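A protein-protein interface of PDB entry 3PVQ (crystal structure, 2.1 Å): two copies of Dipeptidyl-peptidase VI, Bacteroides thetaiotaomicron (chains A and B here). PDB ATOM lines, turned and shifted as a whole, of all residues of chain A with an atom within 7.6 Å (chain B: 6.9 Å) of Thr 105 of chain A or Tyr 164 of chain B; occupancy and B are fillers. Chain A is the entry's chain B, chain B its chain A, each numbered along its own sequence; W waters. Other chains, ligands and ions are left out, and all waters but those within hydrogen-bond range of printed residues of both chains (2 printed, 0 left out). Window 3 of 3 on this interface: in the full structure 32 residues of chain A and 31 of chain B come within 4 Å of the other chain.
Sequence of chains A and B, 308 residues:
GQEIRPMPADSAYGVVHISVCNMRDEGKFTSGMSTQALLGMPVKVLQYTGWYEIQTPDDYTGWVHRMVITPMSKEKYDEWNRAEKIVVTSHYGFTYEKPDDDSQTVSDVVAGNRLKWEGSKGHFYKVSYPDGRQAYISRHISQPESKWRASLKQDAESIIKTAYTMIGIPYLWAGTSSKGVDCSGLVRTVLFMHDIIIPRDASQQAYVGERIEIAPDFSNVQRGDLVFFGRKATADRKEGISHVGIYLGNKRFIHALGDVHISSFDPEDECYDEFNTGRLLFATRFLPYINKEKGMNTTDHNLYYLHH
The backbone carbonyl oxygen of Tyr 164 of chain B is in hydrogen-bond range of the side-chain amide nitrogen of Gln 104 of chain A (2.9 Å).
The backbone carbonyl oxygen of Val 106 of chain A sits close to the backbone carbonyl oxygen of Ile 167 of chain B (3.3 Å).
The backbone NH of Val 106 of chain A sits at hydrogen-bond distance from the backbone carbonyl oxygen of Thr 95 of chain A (2.9 Å).
N of Gly 168 of chain B lies within hydrogen-bond range of O of Val 260 of chain B, 2.8 Å away.
O of Ser 107 of chain A sits at hydrogen-bond distance from N of Thr 95 of chain A.
The backbone carbonyl oxygen (O) of Gln 104 of chain A is in hydrogen-bond range of the backbone NH (N) of Glu 97 of chain A (2.9 Å).
OH of Tyr 129 of chain A is in hydrogen-bond range of OG of Ser 107 of chain A (2.6 Å).
The side-chain hydroxyl (OG1) of Thr 165 of chain B sits at hydrogen-bond distance from the backbone carbonyl oxygen (O) of Thr 162 of chain B, 2.7 Å away.
His 91 of chain B touches Phe 94 of chain A (CD2 to CZ, 3.7 Å).
Thr 165 of chain B touches Phe 94 of chain A (O to CE2, 3.9 Å).
Gln 104 of chain A touches Ile 167 of chain B.
Tyr 164 of chain B touches Thr 105 of chain A.
Thr 105 of chain A touches Thr 165 of chain B (OG1 to O, 3.8 Å).
O of Val 106 of chain A touches CA of Gly 168 of chain B, at 3.4 Å.
Ser 107 of chain A touches Ile 167 of chain B (CA to O, 3.5 Å).
O of Gly 168 of chain B touches CB of Ser 107 of chain A, 3.8 Å away.
Asp 108 of chain A touches Gly 168 of chain B.
Printed residues of chain B within 4 Å of Phe 94 of chain A: His 91 (3.7 Å) and Thr 165 (3.9 Å).
Printed residues of chain B within 4 Å of Gln 104 of chain A: Tyr 164 (2.9 Å) and Ile 167 (3.9 Å).
Printed residues of chain B within 4 Å of Asp 108 of chain A: Gly 168 (3.6 Å).
Of the printed residues of chain A, His 91 of chain B touches Phe 94 (3.7 Å).
No residue of chain A comes within 4 Å of Ala 163 of chain B.
Printed residues of chain A within 4 Å of Tyr 164 of chain B: Gln 104 and Thr 105.
Of the printed residues of chain A, Gly 168 of chain B touches Val 106, Ser 107 and Asp 108.
The nearest printed residue of chain B that does not touch Thr 105 of chain A is Ile 167 of chain B (4.1 Å).
The nearest printed residue of chain A that does not touch Tyr 164 of chain B is Val 106 of chain A (6.9 Å).
The nearest printed residue of chain B that does not touch Val 106 of chain A is Val 260 of chain B (5.8 Å).
Of the 17 printed residues of chain A, 6 touch a printed residue of chain B.
Hydrophobic or aromatic side chains of chain A that line the printed part of chain B: Phe 94.
Along chain A the printed residues that touch a printed residue of chain B span positions 94 to 108.
Hydrophobic or aromatic side chains of chain B within 4 Å of the printed part of chain A: His 91, Tyr 164 and Ile 167.
Along chain B the printed residues that touch a printed residue of chain A span positions 91 to 168.
No position is printed for both chains.
Of the 11 pairs that touch across the chains among the printed residues, none has its exchanged pair printed and touching as well.
Water W2 lies within hydrogen-bond range of the backbone carbonyl oxygen of Ile 167 of chain B (2.6 Å), the side-chain hydroxyl of Thr 105 of chain A (2.7 Å) and the backbone carbonyl oxygen of Thr 165 of chain B (2.8 Å).
Water W1 lies within hydrogen-bond range of the backbone carbonyl oxygen (O) of Gly 168 of chain B (2.7 Å) and the side-chain carboxylate (OD1) of Asp 108 of chain A (2.8 Å).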
ATOM      1  N   GLY A  93     -18.194  10.287 -17.443  1.00  0.00           N
ATOM      2  CA  GLY A  93     -17.524   9.442 -16.463  1.00  0.00           C
ATOM      3  C   GLY A  93     -17.503  10.047 -15.091  1.00  0.00           C
ATOM      4  O   GLY A  93     -18.137  11.078 -14.849  1.00  0.00           O
ATOM      5  N   PHE A  94     -16.733   9.421 -14.206  1.00  0.00           N
ATOM      6  CA  PHE A  94     -16.562   9.837 -12.810  1.00  0.00           C
ATOM      7  C   PHE A  94     -15.118   9.756 -12.393  1.00  0.00           C
ATOM      8  O   PHE A  94     -14.327   9.068 -13.045  1.00  0.00           O
ATOM      9  CB  PHE A  94     -17.417   8.955 -11.852  1.00  0.00           C
ATOM     10  CG  PHE A  94     -18.916   9.164 -11.956  1.00  0.00           C
ATOM     11  CD1 PHE A  94     -19.675   8.441 -12.871  1.00  0.00           C
ATOM     12  CD2 PHE A  94     -19.562  10.096 -11.156  1.00  0.00           C
ATOM     13  CE1 PHE A  94     -21.067   8.643 -12.983  1.00  0.00           C
ATOM     14  CE2 PHE A  94     -20.949  10.304 -11.263  1.00  0.00           C
ATOM     15  CZ  PHE A  94     -21.692   9.574 -12.180  1.00  0.00           C
ATOM     16  N   THR A  95     -14.785  10.451 -11.289  1.00  0.00           N
ATOM     17  CA  THR A  95     -13.487  10.387 -10.593  1.00  0.00           C
ATOM     18  C   THR A  95     -13.787   9.749  -9.254  1.00  0.00           C
ATOM     19  O   THR A  95     -14.926   9.859  -8.777  1.00  0.00           O
ATOM     20  CB  THR A  95     -12.776  11.734 -10.462  1.00  0.00           C
ATOM     21  OG1 THR A  95     -13.511  12.604  -9.598  1.00  0.00           O
ATOM     22  CG2 THR A  95     -12.449  12.377 -11.806  1.00  0.00           C
ATOM     23  N   TYR A  96     -12.803   9.062  -8.654  1.00  0.00           N
ATOM     24  CA  TYR A  96     -13.028   8.329  -7.401  1.00  0.00           C
ATOM     25  C   TYR A  96     -12.063   8.743  -6.330  1.00  0.00           C
ATOM     26  O   TYR A  96     -10.998   9.283  -6.623  1.00  0.00           O
ATOM     27  CB  TYR A  96     -12.921   6.816  -7.656  1.00  0.00           C
ATOM     28  CG  TYR A  96     -13.872   6.335  -8.730  1.00  0.00           C
ATOM     29  CD1 TYR A  96     -15.177   5.966  -8.417  1.00  0.00           C
ATOM     30  CD2 TYR A  96     -13.489   6.309 -10.071  1.00  0.00           C
ATOM     31  CE1 TYR A  96     -16.076   5.585  -9.408  1.00  0.00           C
ATOM     32  CE2 TYR A  96     -14.389   5.951 -11.072  1.00  0.00           C
ATOM     33  CZ  TYR A  96     -15.674   5.576 -10.733  1.00  0.00           C
ATOM     34  OH  TYR A  96     -16.542   5.185 -11.721  1.00  0.00           O
ATOM     35  N   GLU A  97     -12.414   8.444  -5.081  1.00  0.00           N
ATOM     36  CA  GLU A  97     -11.571   8.744  -3.925  1.00  0.00           C
ATOM     37  C   GLU A  97     -10.379   7.786  -3.849  1.00  0.00           C
ATOM     38  O   GLU A  97      -9.350   8.139  -3.297  1.00  0.00           O
ATOM     39  CB  GLU A  97     -12.399   8.643  -2.643  1.00  0.00           C
ATOM     40  CG  GLU A  97     -13.343   9.811  -2.456  1.00  0.00           C
ATOM     41  CD  GLU A  97     -14.047   9.830  -1.115  1.00  0.00           C
ATOM     42  OE1 GLU A  97     -13.876   8.867  -0.337  1.00  0.00           O
ATOM     43  OE2 GLU A  97     -14.811  10.787  -0.860  1.00  0.00           O
ATOM     44  N   LYS A  98     -10.539   6.575  -4.403  1.00  0.00           N
ATOM     45  CA  LYS A  98      -9.532   5.502  -4.413  1.00  0.00           C
ATOM     46  C   LYS A  98      -9.323   4.989  -5.849  1.00  0.00           C
ATOM     47  O   LYS A  98     -10.258   5.116  -6.651  1.00  0.00           O
ATOM     48  CB  LYS A  98     -10.029   4.322  -3.534  1.00  0.00           C
ATOM     49  CG  LYS A  98     -10.106   4.562  -2.035  1.00  0.00           C
ATOM     50  CD  LYS A  98     -10.738   3.330  -1.362  1.00  0.00           C
ATOM     51  CE  LYS A  98     -10.904   3.456   0.133  1.00  0.00           C
ATOM     52  NZ  LYS A  98     -11.562   2.244   0.718  1.00  0.00           N
ATOM     53  N   ASP A 100     -10.183   2.619  -7.562  1.00  0.00           N
ATOM     54  CA  ASP A 100     -11.207   1.571  -7.551  1.00  0.00           C
ATOM     55  C   ASP A 100     -12.496   2.215  -8.016  1.00  0.00           C
ATOM     56  O   ASP A 100     -12.933   3.196  -7.414  1.00  0.00           O
ATOM     57  CB  ASP A 100     -11.339   0.997  -6.115  1.00  0.00           C
ATOM     58  CG  ASP A 100     -12.206  -0.248  -5.958  1.00  0.00           C
ATOM     59  OD1 ASP A 100     -13.091  -0.474  -6.810  1.00  0.00           O
ATOM     60  OD2 ASP A 100     -12.021  -0.975  -4.963  1.00  0.00           O
ATOM     61  N   ASP A 101     -13.111   1.694  -9.084  1.00  0.00           N
ATOM     62  CA  ASP A 101     -14.337   2.302  -9.603  1.00  0.00           C
ATOM     63  C   ASP A 101     -15.577   1.933  -8.758  1.00  0.00           C
ATOM     64  O   ASP A 101     -16.687   2.363  -9.079  1.00  0.00           O
ATOM     65  CB  ASP A 101     -14.551   1.989 -11.100  1.00  0.00           C
ATOM     66  CG  ASP A 101     -14.780   0.538 -11.475  1.00  0.00           C
ATOM     67  OD1 ASP A 101     -14.877  -0.313 -10.554  1.00  0.00           O
ATOM     68  OD2 ASP A 101     -14.903   0.254 -12.694  1.00  0.00           O
ATOM     69  N   ASP A 102     -15.376   1.189  -7.666  1.00  0.00           N
ATOM     70  CA  ASP A 102     -16.434   0.842  -6.721  1.00  0.00           C
ATOM     71  C   ASP A 102     -16.352   1.734  -5.472  1.00  0.00           C
ATOM     72  O   ASP A 102     -17.195   1.610  -4.583  1.00  0.00           O
ATOM     73  CB  ASP A 102     -16.368  -0.654  -6.344  1.00  0.00           C
ATOM     74  CG  ASP A 102     -16.776  -1.592  -7.472  1.00  0.00           C
ATOM     75  OD1 ASP A 102     -17.727  -1.253  -8.217  1.00  0.00           O
ATOM     76  OD2 ASP A 102     -16.159  -2.674  -7.597  1.00  0.00           O
ATOM     77  N   SER A 103     -15.347   2.638  -5.410  1.00  0.00           N
ATOM     78  CA  SER A 103     -15.178   3.538  -4.274  1.00  0.00           C
ATOM     79  C   SER A 103     -16.016   4.807  -4.477  1.00  0.00           C
ATOM     80  O   SER A 103     -16.518   5.043  -5.573  1.00  0.00           O
ATOM     81  CB  SER A 103     -13.704   3.878  -4.057  1.00  0.00           C
ATOM     82  OG  SER A 103     -13.165   4.655  -5.114  1.00  0.00           O
ATOM     83  N   GLN A 104     -16.186   5.600  -3.412  1.00  0.00           N
ATOM     84  CA  GLN A 104     -16.957   6.836  -3.429  1.00  0.00           C
ATOM     85  C   GLN A 104     -16.461   7.784  -4.523  1.00  0.00           C
ATOM     86  O   GLN A 104     -15.267   8.070  -4.594  1.00  0.00           O
ATOM     87  CB  GLN A 104     -16.865   7.520  -2.043  1.00  0.00           C
ATOM     88  CG  GLN A 104     -17.492   8.929  -1.983  1.00  0.00           C
ATOM     89  CD  GLN A 104     -18.978   8.937  -2.277  1.00  0.00           C
ATOM     90  OE1 GLN A 104     -19.748   8.300  -1.591  1.00  0.00           O
ATOM     91  NE2 GLN A 104     -19.410   9.661  -3.290  1.00  0.00           N
ATOM     92  N   THR A 105     -17.390   8.306  -5.338  1.00  0.00           N
ATOM     93  CA  THR A 105     -17.045   9.263  -6.382  1.00  0.00           C
ATOM     94  C   THR A 105     -16.700  10.637  -5.790  1.00  0.00           C
ATOM     95  O   THR A 105     -17.124  10.957  -4.682  1.00  0.00           O
ATOM     96  CB  THR A 105     -18.178   9.404  -7.395  1.00  0.00           C
ATOM     97  OG1 THR A 105     -19.398   9.599  -6.690  1.00  0.00           O
ATOM     98  CG2 THR A 105     -18.289   8.214  -8.329  1.00  0.00           C
ATOM     99  N   VAL A 106     -15.940  11.446  -6.550  1.00  0.00           N
ATOM    100  CA  VAL A 106     -15.553  12.822  -6.198  1.00  0.00           C
ATOM    101  C   VAL A 106     -16.414  13.746  -7.066  1.00  0.00           C
ATOM    102  O   VAL A 106     -17.081  14.635  -6.542  1.00  0.00           O
ATOM    103  CB  VAL A 106     -14.021  13.056  -6.309  1.00  0.00           C
ATOM    104  CG1 VAL A 106     -13.653  14.549  -6.358  1.00  0.00           C
ATOM    105  CG2 VAL A 106     -13.310  12.375  -5.141  1.00  0.00           C
ATOM    106  N   SER A 107     -16.471  13.490  -8.368  1.00  0.00           N
ATOM    107  CA  SER A 107     -17.385  14.225  -9.235  1.00  0.00           C
ATOM    108  C   SER A 107     -17.606  13.463 -10.534  1.00  0.00           C
ATOM    109  O   SER A 107     -16.950  12.449 -10.802  1.00  0.00           O
ATOM    110  CB  SER A 107     -16.884  15.653  -9.504  1.00  0.00           C
ATOM    111  OG  SER A 107     -15.984  15.741 -10.597  1.00  0.00           O
ATOM    112  N   ASP A 108     -18.537  13.947 -11.333  1.00  0.00           N
ATOM    113  CA  ASP A 108     -18.685  13.484 -12.695  1.00  0.00           C
ATOM    114  C   ASP A 108     -17.606  14.244 -13.519  1.00  0.00           C
ATOM    115  O   ASP A 108     -17.049  15.259 -13.054  1.00  0.00           O
ATOM    116  CB  ASP A 108     -20.096  13.778 -13.225  1.00  0.00           C
ATOM    117  CG  ASP A 108     -20.358  15.276 -13.321  1.00  0.00           C
ATOM    118  OD1 ASP A 108     -20.089  15.992 -12.322  1.00  0.00           O
ATOM    119  OD2 ASP A 108     -20.681  15.748 -14.433  1.00  0.00           O
ATOM    120  N   TYR A 129      -8.032  18.705  -8.355  1.00  0.00           N
ATOM    121  CA  TYR A 129      -8.959  19.727  -8.837  1.00  0.00           C
ATOM    122  C   TYR A 129      -8.389  21.104  -8.536  1.00  0.00           C
ATOM    123  O   TYR A 129      -7.565  21.221  -7.606  1.00  0.00           O
ATOM    124  CB  TYR A 129     -10.329  19.538  -8.116  1.00  0.00           C
ATOM    125  CG  TYR A 129     -11.171  18.389  -8.624  1.00  0.00           C
ATOM    126  CD1 TYR A 129     -10.758  17.067  -8.462  1.00  0.00           C
ATOM    127  CD2 TYR A 129     -12.385  18.619  -9.276  1.00  0.00           C
ATOM    128  CE1 TYR A 129     -11.505  16.007  -8.971  1.00  0.00           C
ATOM    129  CE2 TYR A 129     -13.180  17.562  -9.717  1.00  0.00           C
ATOM    130  CZ  TYR A 129     -12.727  16.257  -9.576  1.00  0.00           C
ATOM    131  OH  TYR A 129     -13.476  15.203 -10.030  1.00  0.00           O
ATOM    132  N   ALA A 135      -8.324  13.024  -6.486  1.00  0.00           N
ATOM    133  CA  ALA A 135      -9.135  11.931  -6.975  1.00  0.00           C
ATOM    134  C   ALA A 135      -8.313  11.004  -7.849  1.00  0.00           C
ATOM    135  O   ALA A 135      -7.127  11.254  -8.062  1.00  0.00           O
ATOM    136  CB  ALA A 135     -10.338  12.469  -7.755  1.00  0.00           C
ATOM    137  N   HIS B  91     -26.091   6.382 -13.832  1.00  0.00           N
ATOM    138  CA  HIS B  91     -26.236   7.823 -14.083  1.00  0.00           C
ATOM    139  C   HIS B  91     -26.114   8.165 -15.562  1.00  0.00           C
ATOM    140  O   HIS B  91     -26.957   8.903 -16.058  1.00  0.00           O
ATOM    141  CB  HIS B  91     -25.220   8.664 -13.275  1.00  0.00           C
ATOM    142  CG  HIS B  91     -25.579   8.731 -11.812  1.00  0.00           C
ATOM    143  ND1 HIS B  91     -26.789   9.248 -11.385  1.00  0.00           N
ATOM    144  CD2 HIS B  91     -24.891   8.293 -10.735  1.00  0.00           C
ATOM    145  CE1 HIS B  91     -26.791   9.112 -10.072  1.00  0.00           C
ATOM    146  NE2 HIS B  91     -25.669   8.550  -9.638  1.00  0.00           N
ATOM    147  N   ILE B 159     -32.098   5.605  -0.182  1.00  0.00           N
ATOM    148  CA  ILE B 159     -32.151   6.940  -0.786  1.00  0.00           C
ATOM    149  C   ILE B 159     -30.826   7.713  -0.533  1.00  0.00           C
ATOM    150  O   ILE B 159     -30.337   8.378  -1.452  1.00  0.00           O
ATOM    151  CB  ILE B 159     -33.436   7.687  -0.291  1.00  0.00           C
ATOM    152  CG1 ILE B 159     -34.608   7.452  -1.278  1.00  0.00           C
ATOM    153  CG2 ILE B 159     -33.249   9.198  -0.030  1.00  0.00           C
ATOM    154  CD1 ILE B 159     -35.417   6.270  -1.045  1.00  0.00           C
ATOM    155  N   ILE B 160     -30.228   7.589   0.681  1.00  0.00           N
ATOM    156  CA  ILE B 160     -28.960   8.263   1.019  1.00  0.00           C
ATOM    157  C   ILE B 160     -27.803   7.666   0.178  1.00  0.00           C
ATOM    158  O   ILE B 160     -26.965   8.412  -0.331  1.00  0.00           O
ATOM    159  CB  ILE B 160     -28.699   8.165   2.542  1.00  0.00           C
ATOM    160  CG1 ILE B 160     -29.659   9.101   3.313  1.00  0.00           C
ATOM    161  CG2 ILE B 160     -27.218   8.439   2.898  1.00  0.00           C
ATOM    162  CD1 ILE B 160     -29.718   8.806   4.819  1.00  0.00           C
ATOM    163  N   LYS B 161     -27.780   6.333   0.033  1.00  0.00           N
ATOM    164  CA  LYS B 161     -26.800   5.602  -0.779  1.00  0.00           C
ATOM    165  C   LYS B 161     -26.820   6.157  -2.219  1.00  0.00           C
ATOM    166  O   LYS B 161     -25.760   6.477  -2.758  1.00  0.00           O
ATOM    167  CB  LYS B 161     -27.132   4.100  -0.747  1.00  0.00           C
ATOM    168  CG  LYS B 161     -25.978   3.193  -1.135  1.00  0.00           C
ATOM    169  CD  LYS B 161     -26.421   1.740  -1.348  1.00  0.00           C
ATOM    170  CE  LYS B 161     -25.299   0.926  -1.966  1.00  0.00           C
ATOM    171  NZ  LYS B 161     -25.777  -0.349  -2.554  1.00  0.00           N
ATOM    172  N   THR B 162     -28.033   6.363  -2.801  1.00  0.00           N
ATOM    173  CA  THR B 162     -28.154   6.963  -4.134  1.00  0.00           C
ATOM    174  C   THR B 162     -27.640   8.408  -4.114  1.00  0.00           C
ATOM    175  O   THR B 162     -26.900   8.793  -5.022  1.00  0.00           O
ATOM    176  CB  THR B 162     -29.593   6.904  -4.659  1.00  0.00           C
ATOM    177  OG1 THR B 162     -29.976   5.548  -4.789  1.00  0.00           O
ATOM    178  CG2 THR B 162     -29.748   7.577  -6.027  1.00  0.00           C
ATOM    179  N   ALA B 163     -28.028   9.205  -3.092  1.00  0.00           N
ATOM    180  CA  ALA B 163     -27.611  10.606  -3.001  1.00  0.00           C
ATOM    181  C   ALA B 163     -26.085  10.735  -2.994  1.00  0.00           C
ATOM    182  O   ALA B 163     -25.563  11.626  -3.665  1.00  0.00           O
ATOM    183  CB  ALA B 163     -28.204  11.260  -1.768  1.00  0.00           C
ATOM    184  N   TYR B 164     -25.369   9.797  -2.294  1.00  0.00           N
ATOM    185  CA  TYR B 164     -23.905   9.786  -2.248  1.00  0.00           C
ATOM    186  C   TYR B 164     -23.282   9.524  -3.641  1.00  0.00           C
ATOM    187  O   TYR B 164     -22.191  10.017  -3.882  1.00  0.00           O
ATOM    188  CB  TYR B 164     -23.381   8.750  -1.237  1.00  0.00           C
ATOM    189  CG  TYR B 164     -23.190   9.300   0.162  1.00  0.00           C
ATOM    190  CD1 TYR B 164     -21.980   9.855   0.554  1.00  0.00           C
ATOM    191  CD2 TYR B 164     -24.193   9.188   1.118  1.00  0.00           C
ATOM    192  CE1 TYR B 164     -21.777  10.293   1.866  1.00  0.00           C
ATOM    193  CE2 TYR B 164     -24.016   9.654   2.416  1.00  0.00           C
ATOM    194  CZ  TYR B 164     -22.817  10.226   2.783  1.00  0.00           C
ATOM    195  OH  TYR B 164     -22.678  10.693   4.062  1.00  0.00           O
ATOM    196  N   THR B 165     -23.997   8.811  -4.581  1.00  0.00           N
ATOM    197  CA  THR B 165     -23.439   8.531  -5.912  1.00  0.00           C
ATOM    198  C   THR B 165     -23.495   9.817  -6.792  1.00  0.00           C
ATOM    199  O   THR B 165     -22.975   9.846  -7.918  1.00  0.00           O
ATOM    200  CB  THR B 165     -24.145   7.333  -6.605  1.00  0.00           C
ATOM    201  OG1 THR B 165     -25.471   7.687  -6.978  1.00  0.00           O
ATOM    202  CG2 THR B 165     -24.144   6.066  -5.769  1.00  0.00           C
ATOM    203  N   MET B 166     -24.114  10.878  -6.262  1.00  0.00           N
ATOM    204  CA  MET B 166     -24.301  12.119  -7.011  1.00  0.00           C
ATOM    205  C   MET B 166     -23.380  13.261  -6.560  1.00  0.00           C
ATOM    206  O   MET B 166     -23.454  14.365  -7.109  1.00  0.00           O
ATOM    207  CB  MET B 166     -25.764  12.523  -6.910  1.00  0.00           C
ATOM    208  CG  MET B 166     -26.652  11.521  -7.656  1.00  0.00           C
ATOM    209  SD  MET B 166     -28.329  12.234  -8.118  1.00  0.00           S
ATOM    210  CE  MET B 166     -27.775  13.620  -9.387  1.00  0.00           C
ATOM    211  N   ILE B 167     -22.496  12.992  -5.584  1.00  0.00           N
ATOM    212  CA  ILE B 167     -21.553  13.978  -5.087  1.00  0.00           C
ATOM    213  C   ILE B 167     -20.673  14.523  -6.228  1.00  0.00           C
ATOM    214  O   ILE B 167     -20.175  13.770  -7.093  1.00  0.00           O
ATOM    215  CB  ILE B 167     -20.712  13.404  -3.920  1.00  0.00           C
ATOM    216  CG1 ILE B 167     -21.604  13.410  -2.640  1.00  0.00           C
ATOM    217  CG2 ILE B 167     -19.356  14.205  -3.689  1.00  0.00           C
ATOM    218  CD1 ILE B 167     -21.062  12.671  -1.523  1.00  0.00           C
ATOM    219  N   GLY B 168     -20.557  15.843  -6.225  1.00  0.00           N
ATOM    220  CA  GLY B 168     -19.753  16.602  -7.169  1.00  0.00           C
ATOM    221  C   GLY B 168     -20.463  16.983  -8.442  1.00  0.00           C
ATOM    222  O   GLY B 168     -19.952  17.821  -9.190  1.00  0.00           O
ATOM    223  N   VAL B 190     -32.830  11.622  -7.145  1.00  0.00           N
ATOM    224  CA  VAL B 190     -32.539  10.532  -6.234  1.00  0.00           C
ATOM    225  C   VAL B 190     -33.828   9.700  -6.029  1.00  0.00           C
ATOM    226  O   VAL B 190     -33.805   8.480  -6.165  1.00  0.00           O
ATOM    227  CB  VAL B 190     -32.005  11.128  -4.906  1.00  0.00           C
ATOM    228  CG1 VAL B 190     -32.178  10.156  -3.731  1.00  0.00           C
ATOM    229  CG2 VAL B 190     -30.553  11.611  -5.065  1.00  0.00           C
ATOM    230  N   ARG B 223     -32.162  10.302   9.536  1.00  0.00           N
ATOM    231  CA  ARG B 223     -31.543  10.093   8.226  1.00  0.00           C
ATOM    232  C   ARG B 223     -32.651   9.955   7.205  1.00  0.00           C
ATOM    233  O   ARG B 223     -33.629   9.265   7.484  1.00  0.00           O
ATOM    234  CB  ARG B 223     -30.669   8.819   8.283  1.00  0.00           C
ATOM    235  CG  ARG B 223     -29.329   9.059   8.975  1.00  0.00           C
ATOM    236  CD  ARG B 223     -28.376   7.879   9.098  1.00  0.00           C
ATOM    237  NE  ARG B 223     -28.118   7.150   7.841  1.00  0.00           N
ATOM    238  CZ  ARG B 223     -27.127   7.389   6.977  1.00  0.00           C
ATOM    239  NH1 ARG B 223     -26.308   8.422   7.156  1.00  0.00           N
ATOM    240  NH2 ARG B 223     -26.971   6.618   5.913  1.00  0.00           N
ATOM    241  N   LEU B 248     -28.545  13.488   6.781  1.00  0.00           N
ATOM    242  CA  LEU B 248     -27.689  12.294   6.808  1.00  0.00           C
ATOM    243  C   LEU B 248     -27.418  11.793   8.208  1.00  0.00           C
ATOM    244  O   LEU B 248     -26.699  10.810   8.369  1.00  0.00           O
ATOM    245  CB  LEU B 248     -26.322  12.636   6.164  1.00  0.00           C
ATOM    246  CG  LEU B 248     -26.328  13.074   4.689  1.00  0.00           C
ATOM    247  CD1 LEU B 248     -24.933  13.420   4.241  1.00  0.00           C
ATOM    248  CD2 LEU B 248     -26.968  12.009   3.780  1.00  0.00           C
ATOM    249  N   ARG B 252     -25.335  16.544   9.678  1.00  0.00           N
ATOM    250  CA  ARG B 252     -24.874  16.696   8.308  1.00  0.00           C
ATOM    251  C   ARG B 252     -26.034  16.525   7.310  1.00  0.00           C
ATOM    252  O   ARG B 252     -27.036  15.873   7.615  1.00  0.00           O
ATOM    253  CB  ARG B 252     -23.734  15.719   8.010  1.00  0.00           C
ATOM    254  CG  ARG B 252     -22.505  15.964   8.893  1.00  0.00           C
ATOM    255  CD  ARG B 252     -21.269  15.386   8.274  1.00  0.00           C
ATOM    256  NE  ARG B 252     -20.148  15.441   9.211  1.00  0.00           N
ATOM    257  CZ  ARG B 252     -18.933  14.974   8.950  1.00  0.00           C
ATOM    258  NH1 ARG B 252     -18.671  14.399   7.780  1.00  0.00           N
ATOM    259  NH2 ARG B 252     -17.969  15.074   9.855  1.00  0.00           N
ATOM    260  N   ILE B 254     -26.886  16.506   2.701  1.00  0.00           N
ATOM    261  CA  ILE B 254     -26.403  16.539   1.327  1.00  0.00           C
ATOM    262  C   ILE B 254     -27.338  17.479   0.583  1.00  0.00           C
ATOM    263  O   ILE B 254     -28.549  17.452   0.796  1.00  0.00           O
ATOM    264  CB  ILE B 254     -26.305  15.125   0.695  1.00  0.00           C
ATOM    265  CG1 ILE B 254     -25.594  15.156  -0.706  1.00  0.00           C
ATOM    266  CG2 ILE B 254     -27.685  14.418   0.626  1.00  0.00           C
ATOM    267  CD1 ILE B 254     -24.918  13.861  -1.044  1.00  0.00           C
ATOM    268  N   VAL B 260     -23.259  19.149  -6.026  1.00  0.00           N
ATOM    269  CA  VAL B 260     -23.825  18.283  -4.993  1.00  0.00           C
ATOM    270  C   VAL B 260     -22.719  18.031  -3.963  1.00  0.00           C
ATOM    271  O   VAL B 260     -21.679  17.460  -4.303  1.00  0.00           O
ATOM    272  CB  VAL B 260     -24.409  16.956  -5.556  1.00  0.00           C
ATOM    273  CG1 VAL B 260     -24.904  16.059  -4.423  1.00  0.00           C
ATOM    274  CG2 VAL B 260     -25.524  17.217  -6.567  1.00  0.00           C
ATOM    275  N   ILE B 262     -21.732  17.581   0.673  1.00  0.00           N
ATOM    276  CA  ILE B 262     -22.136  17.380   2.065  1.00  0.00           C
ATOM    277  C   ILE B 262     -21.775  18.615   2.846  1.00  0.00           C
ATOM    278  O   ILE B 262     -20.684  19.159   2.694  1.00  0.00           O
ATOM    279  CB  ILE B 262     -21.517  16.068   2.640  1.00  0.00           C
ATOM    280  CG1 ILE B 262     -22.189  14.847   1.939  1.00  0.00           C
ATOM    281  CG2 ILE B 262     -21.687  15.949   4.168  1.00  0.00           C
ATOM    282  CD1 ILE B 262     -21.450  13.561   2.082  1.00  0.00           C
HETATM  283  O   HOH W   1     -18.914  18.374 -11.569  1.00  0.00           O
HETATM  284  O   HOH W   2     -20.668  11.462  -8.119  1.00  0.00           O
